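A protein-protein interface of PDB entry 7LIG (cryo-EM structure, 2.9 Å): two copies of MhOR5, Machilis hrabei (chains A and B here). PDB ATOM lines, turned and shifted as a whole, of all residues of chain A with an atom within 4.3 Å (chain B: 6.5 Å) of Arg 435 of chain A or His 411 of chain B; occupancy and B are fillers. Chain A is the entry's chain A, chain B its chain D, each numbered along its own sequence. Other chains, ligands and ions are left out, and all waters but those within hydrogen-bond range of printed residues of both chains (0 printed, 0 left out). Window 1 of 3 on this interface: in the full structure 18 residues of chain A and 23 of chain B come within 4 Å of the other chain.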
ATOM      1  N   TYR A 336     -14.562 -22.160   9.501  1.00  0.00           N
ATOM      2  CA  TYR A 336     -13.683 -21.282   8.738  1.00  0.00           C
ATOM      3  C   TYR A 336     -13.302 -21.895   7.398  1.00  0.00           C
ATOM      4  O   TYR A 336     -13.238 -21.188   6.384  1.00  0.00           O
ATOM      5  CB  TYR A 336     -12.431 -20.959   9.544  1.00  0.00           C
ATOM      6  CG  TYR A 336     -11.367 -20.278   8.729  1.00  0.00           C
ATOM      7  CD1 TYR A 336     -11.572 -19.009   8.215  1.00  0.00           C
ATOM      8  CD2 TYR A 336     -10.157 -20.905   8.468  1.00  0.00           C
ATOM      9  CE1 TYR A 336     -10.602 -18.377   7.467  1.00  0.00           C
ATOM     10  CE2 TYR A 336      -9.178 -20.283   7.721  1.00  0.00           C
ATOM     11  CZ  TYR A 336      -9.407 -19.018   7.223  1.00  0.00           C
ATOM     12  OH  TYR A 336      -8.439 -18.390   6.478  1.00  0.00           O
ATOM     13  N   ALA A 431      -6.677 -18.280  22.674  1.00  0.00           N
ATOM     14  CA  ALA A 431      -6.420 -18.640  21.282  1.00  0.00           C
ATOM     15  C   ALA A 431      -7.693 -18.571  20.446  1.00  0.00           C
ATOM     16  O   ALA A 431      -7.681 -18.064  19.316  1.00  0.00           O
ATOM     17  CB  ALA A 431      -5.803 -20.034  21.210  1.00  0.00           C
ATOM     18  N   ILE A 432      -8.808 -19.058  21.000  1.00  0.00           N
ATOM     19  CA  ILE A 432     -10.092 -19.005  20.306  1.00  0.00           C
ATOM     20  C   ILE A 432     -10.509 -17.560  20.062  1.00  0.00           C
ATOM     21  O   ILE A 432     -10.985 -17.214  18.976  1.00  0.00           O
ATOM     22  CB  ILE A 432     -11.158 -19.781  21.103  1.00  0.00           C
ATOM     23  CG1 ILE A 432     -10.898 -21.281  21.018  1.00  0.00           C
ATOM     24  CG2 ILE A 432     -12.550 -19.501  20.587  1.00  0.00           C
ATOM     25  CD1 ILE A 432     -11.851 -22.102  21.844  1.00  0.00           C
ATOM     26  N   ALA A 433     -10.263 -16.680  21.034  1.00  0.00           N
ATOM     27  CA  ALA A 433     -10.647 -15.281  20.875  1.00  0.00           C
ATOM     28  C   ALA A 433      -9.782 -14.575  19.836  1.00  0.00           C
ATOM     29  O   ALA A 433     -10.296 -13.825  18.997  1.00  0.00           O
ATOM     30  CB  ALA A 433     -10.567 -14.559  22.217  1.00  0.00           C
ATOM     31  N   THR A 434      -8.468 -14.812  19.860  1.00  0.00           N
ATOM     32  CA  THR A 434      -7.602 -14.100  18.923  1.00  0.00           C
ATOM     33  C   THR A 434      -7.731 -14.667  17.514  1.00  0.00           C
ATOM     34  O   THR A 434      -7.328 -14.023  16.539  1.00  0.00           O
ATOM     35  CB  THR A 434      -6.144 -14.128  19.377  1.00  0.00           C
ATOM     36  OG1 THR A 434      -5.358 -13.353  18.466  1.00  0.00           O
ATOM     37  CG2 THR A 434      -5.601 -15.529  19.357  1.00  0.00           C
ATOM     38  N   ARG A 435      -8.284 -15.875  17.378  1.00  0.00           N
ATOM     39  CA  ARG A 435      -8.640 -16.337  16.041  1.00  0.00           C
ATOM     40  C   ARG A 435     -10.007 -15.813  15.625  1.00  0.00           C
ATOM     41  O   ARG A 435     -10.248 -15.565  14.440  1.00  0.00           O
ATOM     42  CB  ARG A 435      -8.613 -17.861  15.972  1.00  0.00           C
ATOM     43  CG  ARG A 435      -7.348 -18.414  15.360  1.00  0.00           C
ATOM     44  CD  ARG A 435      -6.277 -18.566  16.411  1.00  0.00           C
ATOM     45  NE  ARG A 435      -4.961 -18.796  15.839  1.00  0.00           N
ATOM     46  CZ  ARG A 435      -3.860 -18.934  16.563  1.00  0.00           C
ATOM     47  NH1 ARG A 435      -3.927 -18.867  17.883  1.00  0.00           N
ATOM     48  NH2 ARG A 435      -2.696 -19.142  15.969  1.00  0.00           N
ATOM     49  N   ALA A 436     -10.914 -15.631  16.585  1.00  0.00           N
ATOM     50  CA  ALA A 436     -12.260 -15.187  16.247  1.00  0.00           C
ATOM     51  C   ALA A 436     -12.304 -13.692  15.976  1.00  0.00           C
ATOM     52  O   ALA A 436     -13.307 -13.183  15.465  1.00  0.00           O
ATOM     53  CB  ALA A 436     -13.231 -15.552  17.365  1.00  0.00           C
ATOM     54  N   GLN A 437     -11.238 -12.968  16.326  1.00  0.00           N
ATOM     55  CA  GLN A 437     -11.176 -11.548  15.990  1.00  0.00           C
ATOM     56  C   GLN A 437     -11.108 -11.316  14.487  1.00  0.00           C
ATOM     57  O   GLN A 437     -11.505 -10.250  14.007  1.00  0.00           O
ATOM     58  CB  GLN A 437      -9.974 -10.894  16.663  1.00  0.00           C
ATOM     59  CG  GLN A 437     -10.298 -10.174  17.950  1.00  0.00           C
ATOM     60  CD  GLN A 437      -9.179  -9.260  18.385  1.00  0.00           C
ATOM     61  OE1 GLN A 437      -8.163  -9.142  17.704  1.00  0.00           O
ATOM     62  NE2 GLN A 437      -9.358  -8.605  19.523  1.00  0.00           N
ATOM     63  N   ILE A 438     -10.602 -12.288  13.732  1.00  0.00           N
ATOM     64  CA  ILE A 438     -10.580 -12.143  12.274  1.00  0.00           C
ATOM     65  C   ILE A 438     -11.977 -12.394  11.729  1.00  0.00           C
ATOM     66  O   ILE A 438     -12.550 -13.475  11.975  1.00  0.00           O
ATOM     67  CB  ILE A 438      -9.563 -13.110  11.651  1.00  0.00           C
ATOM     68  CG1 ILE A 438      -8.157 -12.786  12.144  1.00  0.00           C
ATOM     69  CG2 ILE A 438      -9.620 -13.033  10.143  1.00  0.00           C
ATOM     70  CD1 ILE A 438      -7.767 -11.344  11.953  1.00  0.00           C
ATOM     71  N   GLU B 246       1.859 -26.203   9.562  1.00  0.00           N
ATOM     72  CA  GLU B 246       0.982 -27.368   9.693  1.00  0.00           C
ATOM     73  C   GLU B 246       1.779 -28.659   9.843  1.00  0.00           C
ATOM     74  O   GLU B 246       1.417 -29.534  10.642  1.00  0.00           O
ATOM     75  CB  GLU B 246       0.044 -27.466   8.492  1.00  0.00           C
ATOM     76  CG  GLU B 246      -1.041 -26.409   8.455  1.00  0.00           C
ATOM     77  CD  GLU B 246      -1.999 -26.516   9.621  1.00  0.00           C
ATOM     78  OE1 GLU B 246      -2.418 -25.462  10.143  1.00  0.00           O
ATOM     79  OE2 GLU B 246      -2.335 -27.652  10.015  1.00  0.00           O
ATOM     80  N   GLY B 406      -0.782 -13.392   4.059  1.00  0.00           N
ATOM     81  CA  GLY B 406      -0.448 -13.106   5.449  1.00  0.00           C
ATOM     82  C   GLY B 406      -1.602 -13.395   6.392  1.00  0.00           C
ATOM     83  O   GLY B 406      -1.432 -14.032   7.442  1.00  0.00           O
ATOM     84  N   LEU B 407      -2.805 -12.957   6.015  1.00  0.00           N
ATOM     85  CA  LEU B 407      -3.975 -13.227   6.847  1.00  0.00           C
ATOM     86  C   LEU B 407      -4.319 -14.713   6.859  1.00  0.00           C
ATOM     87  O   LEU B 407      -4.892 -15.220   7.829  1.00  0.00           O
ATOM     88  CB  LEU B 407      -5.167 -12.398   6.374  1.00  0.00           C
ATOM     89  CG  LEU B 407      -5.422 -11.071   7.090  1.00  0.00           C
ATOM     90  CD1 LEU B 407      -5.688 -11.320   8.558  1.00  0.00           C
ATOM     91  CD2 LEU B 407      -4.273 -10.093   6.915  1.00  0.00           C
ATOM     92  N   ASN B 408      -3.976 -15.434   5.787  1.00  0.00           N
ATOM     93  CA  ASN B 408      -4.139 -16.884   5.804  1.00  0.00           C
ATOM     94  C   ASN B 408      -3.101 -17.549   6.694  1.00  0.00           C
ATOM     95  O   ASN B 408      -3.376 -18.596   7.288  1.00  0.00           O
ATOM     96  CB  ASN B 408      -4.052 -17.444   4.388  1.00  0.00           C
ATOM     97  CG  ASN B 408      -5.364 -17.354   3.649  1.00  0.00           C
ATOM     98  OD1 ASN B 408      -6.272 -16.635   4.062  1.00  0.00           O
ATOM     99  ND2 ASN B 408      -5.474 -18.085   2.547  1.00  0.00           N
ATOM    100  N   LEU B 409      -1.903 -16.968   6.784  1.00  0.00           N
ATOM    101  CA  LEU B 409      -0.902 -17.428   7.737  1.00  0.00           C
ATOM    102  C   LEU B 409      -1.338 -17.218   9.177  1.00  0.00           C
ATOM    103  O   LEU B 409      -0.915 -17.983  10.050  1.00  0.00           O
ATOM    104  CB  LEU B 409       0.430 -16.717   7.487  1.00  0.00           C
ATOM    105  CG  LEU B 409       1.649 -17.182   8.280  1.00  0.00           C
ATOM    106  CD1 LEU B 409       1.968 -18.621   7.945  1.00  0.00           C
ATOM    107  CD2 LEU B 409       2.839 -16.287   8.017  1.00  0.00           C
ATOM    108  N   CYS B 410      -2.172 -16.211   9.441  1.00  0.00           N
ATOM    109  CA  CYS B 410      -2.746 -16.038  10.775  1.00  0.00           C
ATOM    110  C   CYS B 410      -3.562 -17.237  11.258  1.00  0.00           C
ATOM    111  O   CYS B 410      -3.525 -17.547  12.452  1.00  0.00           O
ATOM    112  CB  CYS B 410      -3.626 -14.785  10.813  1.00  0.00           C
ATOM    113  SG  CYS B 410      -4.423 -14.457  12.399  1.00  0.00           S
ATOM    114  N   HIS B 411      -4.271 -17.932  10.366  1.00  0.00           N
ATOM    115  CA  HIS B 411      -5.108 -19.070  10.736  1.00  0.00           C
ATOM    116  C   HIS B 411      -4.361 -20.396  10.718  1.00  0.00           C
ATOM    117  O   HIS B 411      -5.000 -21.453  10.740  1.00  0.00           O
ATOM    118  CB  HIS B 411      -6.319 -19.175   9.810  1.00  0.00           C
ATOM    119  CG  HIS B 411      -7.334 -18.097  10.003  1.00  0.00           C
ATOM    120  ND1 HIS B 411      -8.216 -18.087  11.061  1.00  0.00           N
ATOM    121  CD2 HIS B 411      -7.619 -17.000   9.264  1.00  0.00           C
ATOM    122  CE1 HIS B 411      -8.996 -17.025  10.970  1.00  0.00           C
ATOM    123  NE2 HIS B 411      -8.654 -16.349   9.890  1.00  0.00           N
ATOM    124  N   ALA B 412      -3.037 -20.376  10.678  1.00  0.00           N
ATOM    125  CA  ALA B 412      -2.265 -21.602  10.550  1.00  0.00           C
ATOM    126  C   ALA B 412      -2.037 -22.221  11.920  1.00  0.00           C
ATOM    127  O   ALA B 412      -1.811 -21.512  12.904  1.00  0.00           O
ATOM    128  CB  ALA B 412      -0.924 -21.338   9.868  1.00  0.00           C
ATOM    129  N   GLY B 413      -2.102 -23.549  11.977  1.00  0.00           N
ATOM    130  CA  GLY B 413      -1.884 -24.291  13.196  1.00  0.00           C
ATOM    131  C   GLY B 413      -3.105 -24.426  14.079  1.00  0.00           C
ATOM    132  O   GLY B 413      -3.122 -25.293  14.958  1.00  0.00           O
ATOM    133  N   TYR B 414      -4.118 -23.595  13.870  1.00  0.00           N
ATOM    134  CA  TYR B 414      -5.287 -23.593  14.734  1.00  0.00           C
ATOM    135  C   TYR B 414      -6.112 -24.854  14.519  1.00  0.00           C
ATOM    136  O   TYR B 414      -6.880 -24.952  13.560  1.00  0.00           O
ATOM    137  CB  TYR B 414      -6.117 -22.348  14.442  1.00  0.00           C
ATOM    138  CG  TYR B 414      -7.325 -22.171  15.310  1.00  0.00           C
ATOM    139  CD1 TYR B 414      -7.239 -22.296  16.683  1.00  0.00           C
ATOM    140  CD2 TYR B 414      -8.552 -21.862  14.753  1.00  0.00           C
ATOM    141  CE1 TYR B 414      -8.345 -22.126  17.476  1.00  0.00           C
ATOM    142  CE2 TYR B 414      -9.659 -21.689  15.536  1.00  0.00           C
ATOM    143  CZ  TYR B 414      -9.553 -21.824  16.894  1.00  0.00           C
ATOM    144  OH  TYR B 414     -10.666 -21.651  17.676  1.00  0.00           O
ATOM    145  N   SER B 415      -5.950 -25.822  15.421  1.00  0.00           N
ATOM    146  CA  SER B 415      -6.624 -27.107  15.293  1.00  0.00           C
ATOM    147  C   SER B 415      -6.714 -27.811  16.638  1.00  0.00           C
ATOM    148  O   SER B 415      -6.479 -27.199  17.682  1.00  0.00           O
ATOM    149  CB  SER B 415      -5.897 -27.998  14.290  1.00  0.00           C
ATOM    150  OG  SER B 415      -4.619 -28.354  14.779  1.00  0.00           O
ATOM    151  N   LEU B 418      -3.283 -28.168  18.784  1.00  0.00           N
ATOM    152  CA  LEU B 418      -2.795 -27.002  19.516  1.00  0.00           C
ATOM    153  C   LEU B 418      -3.293 -26.994  20.954  1.00  0.00           C
ATOM    154  O   LEU B 418      -2.622 -26.472  21.850  1.00  0.00           O
ATOM    155  CB  LEU B 418      -3.229 -25.730  18.795  1.00  0.00           C
ATOM    156  CG  LEU B 418      -2.762 -24.386  19.338  1.00  0.00           C
ATOM    157  CD1 LEU B 418      -1.362 -24.109  18.859  1.00  0.00           C
ATOM    158  CD2 LEU B 418      -3.707 -23.290  18.903  1.00  0.00           C
ATOM    159  N   ILE B 429       2.933 -20.081  18.949  1.00  0.00           N
ATOM    160  CA  ILE B 429       1.896 -19.977  17.924  1.00  0.00           C
ATOM    161  C   ILE B 429       1.054 -18.728  18.155  1.00  0.00           C
ATOM    162  O   ILE B 429       0.660 -18.041  17.203  1.00  0.00           O
ATOM    163  CB  ILE B 429       1.043 -21.258  17.900  1.00  0.00           C
ATOM    164  CG1 ILE B 429       1.882 -22.441  17.428  1.00  0.00           C
ATOM    165  CG2 ILE B 429      -0.136 -21.118  16.967  1.00  0.00           C
ATOM    166  CD1 ILE B 429       2.543 -22.223  16.102  1.00  0.00           C
ATOM    167  N   GLN B 430       0.822 -18.382  19.423  1.00  0.00           N
ATOM    168  CA  GLN B 430       0.126 -17.142  19.746  1.00  0.00           C
ATOM    169  C   GLN B 430       0.926 -15.926  19.302  1.00  0.00           C
ATOM    170  O   GLN B 430       0.359 -14.969  18.758  1.00  0.00           O
ATOM    171  CB  GLN B 430      -0.150 -17.080  21.246  1.00  0.00           C
ATOM    172  CG  GLN B 430      -0.847 -15.821  21.688  1.00  0.00           C
ATOM    173  CD  GLN B 430      -2.178 -15.650  21.006  1.00  0.00           C
ATOM    174  OE1 GLN B 430      -2.973 -16.582  20.946  1.00  0.00           O
ATOM    175  NE2 GLN B 430      -2.431 -14.458  20.487  1.00  0.00           N
ATOM    176  N   ILE B 432       3.194 -15.860  16.839  1.00  0.00           N
ATOM    177  CA  ILE B 432       3.173 -15.857  15.377  1.00  0.00           C
ATOM    178  C   ILE B 432       1.851 -15.302  14.864  1.00  0.00           C
ATOM    179  O   ILE B 432       1.823 -14.509  13.918  1.00  0.00           O
ATOM    180  CB  ILE B 432       3.450 -17.273  14.840  1.00  0.00           C
ATOM    181  CG1 ILE B 432       4.910 -17.652  15.062  1.00  0.00           C
ATOM    182  CG2 ILE B 432       3.141 -17.378  13.365  1.00  0.00           C
ATOM    183  CD1 ILE B 432       5.235 -19.058  14.637  1.00  0.00           C
ATOM    184  N   ALA B 433       0.745 -15.649  15.524  1.00  0.00           N
ATOM    185  CA  ALA B 433      -0.560 -15.168  15.079  1.00  0.00           C
ATOM    186  C   ALA B 433      -0.721 -13.672  15.326  1.00  0.00           C
ATOM    187  O   ALA B 433      -1.214 -12.940  14.457  1.00  0.00           O
ATOM    188  CB  ALA B 433      -1.671 -15.947  15.775  1.00  0.00           C
ATOM    189  N   THR B 434      -0.298 -13.188  16.497  1.00  0.00           N
ATOM    190  CA  THR B 434      -0.498 -11.771  16.793  1.00  0.00           C
ATOM    191  C   THR B 434       0.486 -10.901  16.019  1.00  0.00           C
ATOM    192  O   THR B 434       0.286  -9.688  15.893  1.00  0.00           O
ATOM    193  CB  THR B 434      -0.391 -11.493  18.292  1.00  0.00           C
ATOM    194  OG1 THR B 434      -0.674 -10.110  18.528  1.00  0.00           O
ATOM    195  CG2 THR B 434       1.000 -11.759  18.790  1.00  0.00           C
ATOM    196  N   ALA B 436       1.181 -11.945  12.803  1.00  0.00           N
ATOM    197  CA  ALA B 436       0.667 -12.111  11.448  1.00  0.00           C
ATOM    198  C   ALA B 436      -0.632 -11.349  11.246  1.00  0.00           C
ATOM    199  O   ALA B 436      -1.092 -11.196  10.110  1.00  0.00           O
ATOM    200  CB  ALA B 436       0.469 -13.591  11.138  1.00  0.00           C
ATOM    201  N   GLN B 437      -1.250 -10.880  12.333  1.00  0.00           N
ATOM    202  CA  GLN B 437      -2.442 -10.046  12.196  1.00  0.00           C
ATOM    203  C   GLN B 437      -2.134  -8.711  11.532  1.00  0.00           C
ATOM    204  O   GLN B 437      -3.022  -8.101  10.930  1.00  0.00           O
ATOM    205  CB  GLN B 437      -3.083  -9.804  13.559  1.00  0.00           C
ATOM    206  CG  GLN B 437      -4.239 -10.722  13.873  1.00  0.00           C
ATOM    207  CD  GLN B 437      -5.053 -10.227  15.042  1.00  0.00           C
ATOM    208  OE1 GLN B 437      -4.767  -9.174  15.606  1.00  0.00           O
ATOM    209  NE2 GLN B 437      -6.076 -10.983  15.415  1.00  0.00           N
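The backbone carbonyl oxygen (O) of Thr 434 of chain A is in hydrogen-bond range of the side-chain amide nitrogen (NE2) of Gln 437 of chain B, 3.5 Å away.
CG1 of Ile 432 of chain A touches OH of Tyr 414 of chain B, at 3.4 Å.
Cys 410 of chain B touches Arg 435 of chain A (O to NE, 3.9 Å).
Arg 435 of chain A touches His 411 of chain B.
O of Ala 412 of chain B touches NH2 of Arg 435 of chain A, at 3.97 Å.
Arg 435 of chain A touches Tyr 414 of chain B.
NH1 of Arg 435 of chain A touches OE1 of Gln 430 of chain B, 3.9 Å away.
Arg 435 of chain A touches Ala 433 of chain B.
Ile 438 of chain A touches Leu 407 of chain B (CD1 to CD1, 3.98 Å).
CG2 of Ile 438 of chain A touches NE2 of His 411 of chain B, 3.5 Å away.
Gln 437 of chain B touches Ile 438 of chain A (NE2 to CD1, 3.9 Å).
Arg 435 of chain A touches just these residues of chain B: Cys 410 (3.9 Å), His 411 (3.97 Å), Ala 412 (3.97 Å), Tyr 414 (3.7 Å), Ile 429 (3.4 Å), Gln 430 (3.9 Å) and Ala 433 (3.4 Å).
His 411 of chain B touches just these residues of chain A: Tyr 336 (3.2 Å), Arg 435 (3.97 Å) and Ile 438 (3.5 Å).
Printed residues of chain A within 4 Å of Ala 433 of chain B: Arg 435.
Of the printed residues of chain A, Gln 437 of chain B touches Thr 434 (3.5 Å), Gln 437 (3.6 Å) and Ile 438 (3.9 Å).
Printed residues of chain A within 4 Å of Cys 410 of chain B: Arg 435 (3.9 Å).
Glu 246 of chain B touches none of the printed residues of chain A.
The nearest printed residue of chain A that does not touch His 411 of chain B is Ala 436 of chain A (6.1 Å).
The nearest printed residue of chain A that does not touch Cys 410 of chain B is Ile 438 of chain A (4.1 Å).
Of the 19 printed residues of chain B, 10 touch a printed residue of chain A.
Hydrophobic or aromatic side chains of chain B within 4 Å of the printed part of chain A: Leu 407, His 411, Tyr 414, Ile 429 and Ala 433.
Of the 9 printed residues of chain A, 6 touch a printed residue of chain B.
Hydrophobic or aromatic side chains of chain A that line the printed part of chain B: Tyr 336, Ile 432 and Ile 438.
Thr 434 of chain A touches Gln 437 of chain B, but with the chains exchanged Gln 437 of chain A does not touch Thr 434 of chain B (7.6 Å).
Gln 437 of chain B touches its own counterpart, Gln 437 of chain A.
Of the 16 pairs that touch across the chains among the printed residues, 1 has its exchanged pair printed and touching as well.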
